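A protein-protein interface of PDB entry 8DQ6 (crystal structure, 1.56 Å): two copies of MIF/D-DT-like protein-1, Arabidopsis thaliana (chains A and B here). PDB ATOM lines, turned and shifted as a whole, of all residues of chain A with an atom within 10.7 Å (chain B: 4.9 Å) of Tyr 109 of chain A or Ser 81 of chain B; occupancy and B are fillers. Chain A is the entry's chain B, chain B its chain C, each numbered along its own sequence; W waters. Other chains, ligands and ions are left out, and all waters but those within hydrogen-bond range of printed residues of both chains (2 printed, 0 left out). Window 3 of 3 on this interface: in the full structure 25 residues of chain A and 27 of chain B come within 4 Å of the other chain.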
ATOM      1  N   SER A  36       1.324  13.389  28.549  1.00  0.00           N
ATOM      2  CA  SER A  36       2.542  14.018  28.048  1.00  0.00           C
ATOM      3  C   SER A  36       3.700  13.917  29.030  1.00  0.00           C
ATOM      4  O   SER A  36       4.861  14.042  28.623  1.00  0.00           O
ATOM      5  CB  SER A  36       2.269  15.489  27.728  1.00  0.00           C
ATOM      6  OG  SER A  36       2.000  16.218  28.918  1.00  0.00           O
ATOM      7  N   MET A  39       6.383   8.410  30.887  1.00  0.00           N
ATOM      8  CA  MET A  39       7.252   7.560  30.082  1.00  0.00           C
ATOM      9  C   MET A  39       7.272   6.180  30.715  1.00  0.00           C
ATOM     10  O   MET A  39       7.417   6.065  31.933  1.00  0.00           O
ATOM     11  CB  MET A  39       8.671   8.145  29.984  1.00  0.00           C
ATOM     12  CG  MET A  39       9.646   7.257  29.214  1.00  0.00           C
ATOM     13  SD  MET A  39      11.341   7.888  29.281  1.00  0.00           S
ATOM     14  CE  MET A  39      11.280   8.989  27.883  1.00  0.00           C
ATOM     15  N   PRO A 105      13.574  18.623  39.057  1.00  0.00           N
ATOM     16  CA  PRO A 105      12.861  18.203  37.843  1.00  0.00           C
ATOM     17  C   PRO A 105      13.728  17.355  36.921  1.00  0.00           C
ATOM     18  O   PRO A 105      14.958  17.327  37.016  1.00  0.00           O
ATOM     19  CB  PRO A 105      12.484  19.529  37.172  1.00  0.00           C
ATOM     20  CG  PRO A 105      12.575  20.573  38.279  1.00  0.00           C
ATOM     21  CD  PRO A 105      13.689  20.091  39.151  1.00  0.00           C
ATOM     22  N   PHE A 106      13.051  16.638  36.021  1.00  0.00           N
ATOM     23  CA  PHE A 106      13.730  16.045  34.878  1.00  0.00           C
ATOM     24  C   PHE A 106      14.273  17.144  33.971  1.00  0.00           C
ATOM     25  O   PHE A 106      13.827  18.296  34.000  1.00  0.00           O
ATOM     26  CB  PHE A 106      12.783  15.175  34.037  1.00  0.00           C
ATOM     27  CG  PHE A 106      12.206  13.980  34.760  1.00  0.00           C
ATOM     28  CD1 PHE A 106      13.029  13.016  35.318  1.00  0.00           C
ATOM     29  CD2 PHE A 106      10.829  13.806  34.843  1.00  0.00           C
ATOM     30  CE1 PHE A 106      12.488  11.915  35.972  1.00  0.00           C
ATOM     31  CE2 PHE A 106      10.281  12.712  35.495  1.00  0.00           C
ATOM     32  CZ  PHE A 106      11.104  11.766  36.060  1.00  0.00           C
ATOM     33  N   PHE A 107      15.237  16.775  33.144  1.00  0.00           N
ATOM     34  CA  PHE A 107      15.653  17.593  32.012  1.00  0.00           C
ATOM     35  C   PHE A 107      15.044  16.959  30.772  1.00  0.00           C
ATOM     36  O   PHE A 107      15.434  15.853  30.385  1.00  0.00           O
ATOM     37  CB  PHE A 107      17.174  17.658  31.908  1.00  0.00           C
ATOM     38  CG  PHE A 107      17.831  18.298  33.087  1.00  0.00           C
ATOM     39  CD1 PHE A 107      17.999  19.674  33.135  1.00  0.00           C
ATOM     40  CD2 PHE A 107      18.281  17.528  34.148  1.00  0.00           C
ATOM     41  CE1 PHE A 107      18.606  20.269  34.230  1.00  0.00           C
ATOM     42  CE2 PHE A 107      18.891  18.119  35.240  1.00  0.00           C
ATOM     43  CZ  PHE A 107      19.052  19.490  35.282  1.00  0.00           C
ATOM     44  N   GLY A 108      14.076  17.640  30.167  1.00  0.00           N
ATOM     45  CA  GLY A 108      13.363  17.106  29.026  1.00  0.00           C
ATOM     46  C   GLY A 108      13.593  17.962  27.797  1.00  0.00           C
ATOM     47  O   GLY A 108      13.766  19.180  27.895  1.00  0.00           O
ATOM     48  N   TYR A 109      13.601  17.309  26.636  1.00  0.00           N
ATOM     49  CA  TYR A 109      13.822  17.996  25.361  1.00  0.00           C
ATOM     50  C   TYR A 109      12.958  17.393  24.259  1.00  0.00           C
ATOM     51  O   TYR A 109      12.848  16.172  24.147  1.00  0.00           O
ATOM     52  CB  TYR A 109      15.301  17.931  24.972  1.00  0.00           C
ATOM     53  CG  TYR A 109      16.209  18.401  26.085  1.00  0.00           C
ATOM     54  CD1 TYR A 109      16.496  19.748  26.250  1.00  0.00           C
ATOM     55  CD2 TYR A 109      16.746  17.500  26.995  1.00  0.00           C
ATOM     56  CE1 TYR A 109      17.311  20.184  27.286  1.00  0.00           C
ATOM     57  CE2 TYR A 109      17.555  17.923  28.028  1.00  0.00           C
ATOM     58  CZ  TYR A 109      17.836  19.268  28.172  1.00  0.00           C
ATOM     59  OH  TYR A 109      18.653  19.682  29.205  1.00  0.00           O
ATOM     60  N   GLY B  74      22.299  20.655  33.209  1.00  0.00           N
ATOM     61  CA  GLY B  74      21.457  21.131  32.121  1.00  0.00           C
ATOM     62  C   GLY B  74      22.187  21.173  30.790  1.00  0.00           C
ATOM     63  O   GLY B  74      21.660  20.736  29.762  1.00  0.00           O
ATOM     64  N   LEU B  76      24.813  19.409  30.141  1.00  0.00           N
ATOM     65  CA  LEU B  76      25.146  18.019  29.850  1.00  0.00           C
ATOM     66  C   LEU B  76      23.961  17.285  29.233  1.00  0.00           C
ATOM     67  O   LEU B  76      24.089  16.652  28.178  1.00  0.00           O
ATOM     68  CB  LEU B  76      25.595  17.320  31.131  1.00  0.00           C
ATOM     69  CG  LEU B  76      26.099  15.891  31.005  1.00  0.00           C
ATOM     70  CD1 LEU B  76      26.875  15.735  29.706  1.00  0.00           C
ATOM     71  CD2 LEU B  76      26.974  15.573  32.196  1.00  0.00           C
ATOM     72  N   SER B  77      22.806  17.335  29.895  1.00  0.00           N
ATOM     73  CA  SER B  77      21.625  16.653  29.378  1.00  0.00           C
ATOM     74  C   SER B  77      21.234  17.183  28.004  1.00  0.00           C
ATOM     75  O   SER B  77      20.868  16.406  27.118  1.00  0.00           O
ATOM     76  CB  SER B  77      20.469  16.788  30.372  1.00  0.00           C
ATOM     77  OG  SER B  77      19.814  18.035  30.223  1.00  0.00           O
ATOM     78  N   GLU B  78      21.311  18.500  27.803  1.00  0.00           N
ATOM     79  CA  GLU B  78      20.965  19.055  26.498  1.00  0.00           C
ATOM     80  C   GLU B  78      21.966  18.616  25.433  1.00  0.00           C
ATOM     81  O   GLU B  78      21.574  18.310  24.300  1.00  0.00           O
ATOM     82  CB  GLU B  78      20.875  20.583  26.583  1.00  0.00           C
ATOM     83  CG  GLU B  78      21.246  21.334  25.315  1.00  0.00           C
ATOM     84  CD  GLU B  78      22.388  22.312  25.535  1.00  0.00           C
ATOM     85  N   THR B  79      23.257  18.545  25.781  1.00  0.00           N
ATOM     86  CA  THR B  79      24.243  18.091  24.804  1.00  0.00           C
ATOM     87  C   THR B  79      24.019  16.629  24.429  1.00  0.00           C
ATOM     88  O   THR B  79      24.070  16.278  23.246  1.00  0.00           O
ATOM     89  CB  THR B  79      25.663  18.312  25.337  1.00  0.00           C
ATOM     90  OG1 THR B  79      25.870  19.716  25.572  1.00  0.00           O
ATOM     91  CG2 THR B  79      26.696  17.819  24.330  1.00  0.00           C
ATOM     92  N   ILE B  80      23.776  15.757  25.415  1.00  0.00           N
ATOM     93  CA  ILE B  80      23.480  14.363  25.088  1.00  0.00           C
ATOM     94  C   ILE B  80      22.217  14.283  24.242  1.00  0.00           C
ATOM     95  O   ILE B  80      22.150  13.519  23.269  1.00  0.00           O
ATOM     96  CB  ILE B  80      23.363  13.515  26.371  1.00  0.00           C
ATOM     97  CG1 ILE B  80      24.672  13.574  27.159  1.00  0.00           C
ATOM     98  CG2 ILE B  80      23.009  12.077  26.014  1.00  0.00           C
ATOM     99  CD1 ILE B  80      25.897  13.152  26.352  1.00  0.00           C
ATOM    100  N   SER B  81      21.212  15.091  24.580  1.00  0.00           N
ATOM    101  CA  SER B  81      19.990  15.111  23.788  1.00  0.00           C
ATOM    102  C   SER B  81      20.292  15.480  22.340  1.00  0.00           C
ATOM    103  O   SER B  81      19.788  14.835  21.414  1.00  0.00           O
ATOM    104  CB  SER B  81      18.985  16.087  24.404  1.00  0.00           C
ATOM    105  OG  SER B  81      17.840  16.213  23.584  1.00  0.00           O
ATOM    106  N   GLU B  82      21.159  16.481  22.123  1.00  0.00           N
ATOM    107  CA  GLU B  82      21.516  16.858  20.752  1.00  0.00           C
ATOM    108  C   GLU B  82      22.274  15.742  20.035  1.00  0.00           C
ATOM    109  O   GLU B  82      22.025  15.478  18.849  1.00  0.00           O
ATOM    110  CB  GLU B  82      22.328  18.159  20.755  1.00  0.00           C
ATOM    111  CG  GLU B  82      21.454  19.392  20.977  1.00  0.00           C
ATOM    112  CD  GLU B  82      22.226  20.627  21.431  1.00  0.00           C
ATOM    113  OE1 GLU B  82      23.477  20.616  21.388  1.00  0.00           O
ATOM    114  OE2 GLU B  82      21.571  21.619  21.834  1.00  0.00           O
ATOM    115  N   ILE B  83      23.198  15.072  20.731  1.00  0.00           N
ATOM    116  CA  ILE B  83      23.916  13.955  20.122  1.00  0.00           C
ATOM    117  C   ILE B  83      22.941  12.881  19.653  1.00  0.00           C
ATOM    118  O   ILE B  83      23.074  12.343  18.547  1.00  0.00           O
ATOM    119  CB  ILE B  83      24.967  13.397  21.107  1.00  0.00           C
ATOM    120  CG1 ILE B  83      26.123  14.397  21.240  1.00  0.00           C
ATOM    121  CG2 ILE B  83      25.469  12.034  20.658  1.00  0.00           C
ATOM    122  CD1 ILE B  83      26.988  14.194  22.497  1.00  0.00           C
ATOM    123  N   LEU B  84      21.953  12.543  20.489  1.00  0.00           N
ATOM    124  CA  LEU B  84      21.003  11.496  20.127  1.00  0.00           C
ATOM    125  C   LEU B  84      20.100  11.938  18.988  1.00  0.00           C
ATOM    126  O   LEU B  84      19.693  11.112  18.158  1.00  0.00           O
ATOM    127  CB  LEU B  84      20.168  11.100  21.351  1.00  0.00           C
ATOM    128  CG  LEU B  84      21.015  10.528  22.495  1.00  0.00           C
ATOM    129  CD1 LEU B  84      20.143  10.231  23.730  1.00  0.00           C
ATOM    130  CD2 LEU B  84      21.787   9.285  22.047  1.00  0.00           C
ATOM    131  N   GLN B  85      19.774  13.228  18.925  1.00  0.00           N
ATOM    132  CA  GLN B  85      19.006  13.718  17.786  1.00  0.00           C
ATOM    133  C   GLN B  85      19.817  13.602  16.499  1.00  0.00           C
ATOM    134  O   GLN B  85      19.324  13.111  15.476  1.00  0.00           O
ATOM    135  CB  GLN B  85      18.575  15.161  18.035  1.00  0.00           C
ATOM    136  CG  GLN B  85      17.832  15.786  16.875  1.00  0.00           C
ATOM    137  CD  GLN B  85      16.855  16.841  17.332  1.00  0.00           C
ATOM    138  OE1 GLN B  85      15.676  16.798  16.998  1.00  0.00           O
ATOM    139  NE2 GLN B  85      17.344  17.798  18.108  1.00  0.00           N
ATOM    140  N   ILE B  90      16.339  11.028  17.278  1.00  0.00           N
ATOM    141  CA  ILE B  90      15.434  11.007  18.419  1.00  0.00           C
ATOM    142  C   ILE B  90      15.044  12.442  18.746  1.00  0.00           C
ATOM    143  O   ILE B  90      15.905  13.276  19.052  1.00  0.00           O
ATOM    144  CB  ILE B  90      16.078  10.316  19.628  1.00  0.00           C
ATOM    145  CG1 ILE B  90      16.176   8.814  19.379  1.00  0.00           C
ATOM    146  CG2 ILE B  90      15.270  10.582  20.872  1.00  0.00           C
ATOM    147  CD1 ILE B  90      17.114   8.100  20.337  1.00  0.00           C
ATOM    148  N   ASP B  91      13.743  12.728  18.686  1.00  0.00           N
ATOM    149  CA  ASP B  91      13.223  14.062  18.934  1.00  0.00           C
ATOM    150  C   ASP B  91      12.704  14.254  20.353  1.00  0.00           C
ATOM    151  O   ASP B  91      12.380  15.385  20.727  1.00  0.00           O
ATOM    152  CB  ASP B  91      12.097  14.386  17.939  1.00  0.00           C
ATOM    153  CG  ASP B  91      12.610  14.621  16.528  1.00  0.00           C
ATOM    154  OD1 ASP B  91      13.706  15.193  16.378  1.00  0.00           O
ATOM    155  OD2 ASP B  91      11.912  14.240  15.567  1.00  0.00           O
ATOM    156  N   SER B  92      12.620  13.191  21.153  1.00  0.00           N
ATOM    157  CA  SER B  92      12.102  13.276  22.513  1.00  0.00           C
ATOM    158  C   SER B  92      13.055  12.566  23.459  1.00  0.00           C
ATOM    159  O   SER B  92      13.454  11.429  23.199  1.00  0.00           O
ATOM    160  CB  SER B  92      10.712  12.643  22.605  1.00  0.00           C
ATOM    161  OG  SER B  92       9.947  13.247  23.628  1.00  0.00           O
ATOM    162  N   SER B  93      13.418  13.225  24.554  1.00  0.00           N
ATOM    163  CA  SER B  93      14.335  12.616  25.504  1.00  0.00           C
ATOM    164  C   SER B  93      14.065  13.160  26.893  1.00  0.00           C
ATOM    165  O   SER B  93      13.525  14.259  27.053  1.00  0.00           O
ATOM    166  CB  SER B  93      15.791  12.842  25.091  1.00  0.00           C
ATOM    167  OG  SER B  93      16.128  14.208  25.210  1.00  0.00           O
ATOM    168  N   PHE B  95      16.006  13.139  30.938  1.00  0.00           N
ATOM    169  CA  PHE B  95      17.183  12.834  31.737  1.00  0.00           C
ATOM    170  C   PHE B  95      16.882  13.065  33.203  1.00  0.00           C
ATOM    171  O   PHE B  95      16.241  14.058  33.573  1.00  0.00           O
ATOM    172  CB  PHE B  95      18.401  13.672  31.303  1.00  0.00           C
ATOM    173  CG  PHE B  95      18.845  13.379  29.910  1.00  0.00           C
ATOM    174  CD1 PHE B  95      19.859  12.461  29.671  1.00  0.00           C
ATOM    175  CD2 PHE B  95      18.213  13.977  28.825  1.00  0.00           C
ATOM    176  CE1 PHE B  95      20.252  12.172  28.376  1.00  0.00           C
ATOM    177  CE2 PHE B  95      18.605  13.679  27.524  1.00  0.00           C
ATOM    178  CZ  PHE B  95      19.618  12.779  27.306  1.00  0.00           C
HETATM  179  O   HOH W   1      15.162  15.339  22.316  1.00  0.00           O
HETATM  180  O   HOH W   2      10.820  15.681  27.940  1.00  0.00           O
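No position is printed for both chains. Of the 12 pairs that touch across the chains among the printed residues, none has its exchanged pair printed and touching as well.
The backbone NH (N) of Phe 95 of chain B sits at hydrogen-bond distance from the backbone carbonyl oxygen (O) of Phe 107 of chain A, at 2.8 Å. The side-chain hydroxyl of Tyr 109 of chain A lies within hydrogen-bond range of the backbone carbonyl oxygen of Gly 74 of chain B (3.2 Å). OH of Tyr 109 of chain A sits at hydrogen-bond distance from N of Glu 78 of chain B, at 3.2 Å. O of Tyr 109 of chain A is in hydrogen-bond range of N of Ser 93 of chain B (3.0 Å). The side-chain hydroxyl (OG) of Ser 77 of chain B sits close to the side-chain hydroxyl (OH) of Tyr 109 of chain A, 2.3 Å away.
Among the printed residues, merely in contact across the chains: Phe 106 of chain A with Phe 95 of chain B, Phe 107 of chain A with Gly 74 of chain B, Phe 107 of chain A with Ser 77 of chain B, Gly 108 of chain A with Ser 93 of chain B, Tyr 109 of chain A with Ser 81 of chain B, Tyr 109 of chain A with Asp 91 of chain B and Tyr 109 of chain A with Ser 92 of chain B.
Hydrophobic or aromatic side chains of chain A that line the printed part of chain B: Phe 106, Phe 107 and Tyr 109. Hydrophobic or aromatic side chains of chain B that line the printed part of chain A: Phe 95. Among the printed residues, 12 pairs touch across the chains.
Water W1 lies within hydrogen-bond range of O of Tyr 109 of chain A, OG of Ser 81 of chain B, O of Asp 91 of chain B and OG of Ser 93 of chain B. Water W2 lies within hydrogen-bond range of the backbone carbonyl oxygen (O) of Ser 93 of chain B (3.2 Å) and the backbone NH (N) of Tyr 109 of chain A (3.5 Å).
Tyr 109 of chain A touches just these residues of chain B: Gly 74 (3.2 Å), Ser 77 (2.3 Å), Glu 78 (3.2 Å), Ser 81 (3.4 Å), Asp 91 (3.5 Å), Ser 92 (3.4 Å) and Ser 93 (3.0 Å). Of chain A, only Tyr 109 (3.4 Å) comes within 4 Å of Ser 81 of chain B. Ser 77 of chain B touches just these residues of chain A: Phe 107 and Tyr 109. Glu 78 of chain B touches just one residue of chain A: Tyr 109 (3.2 Å). Ile 80 of chain B touches none of the printed residues of chain A. No residue of chain A comes within 4 Å of Glu 82 of chain B. No residue of chain A comes within 4 Å of Leu 84 of chain B. No residue of chain A comes within 4 Å of Gln 85 of chain B. Of the printed residues of chain A, Ser 92 of chain B touches Tyr 109. Of the printed residues of chain B, Phe 106 of chain A touches Phe 95. Printed residues of chain B within 4 Å of Gly 108 of chain A: Ser 93. Of the printed residues of chain A, Phe 95 of chain B touches Phe 106 and Phe 107. Printed residues of chain A within 4 Å of Asp 91 of chain B: Tyr 109. Printed residues of chain B within 4 Å of Phe 107 of chain A: Gly 74 (3.6 Å), Ser 77 (3.2 Å) and Phe 95 (2.8 Å). The nearest residue of chain A that does not touch Ser 81 of chain B is Gly 108 of chain A (6.2 Å). The nearest printed residue of chain A that does not touch Phe 95 of chain B is Tyr 109 of chain A (4.1 Å).
The backbone carbonyl oxygen of Gly 74 of chain B is in hydrogen-bond range of the side-chain hydroxyl of Ser 77 of chain B. The side-chain hydroxyl (OG) of Ser 81 of chain B is in hydrogen-bond range of the side-chain hydroxyl (OG) of Ser 93 of chain B (3.1 Å). The side-chain amide oxygen of Gln 85 of chain B sits close to the side-chain carboxylate of Asp 91 of chain B, at 2.6 Å.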
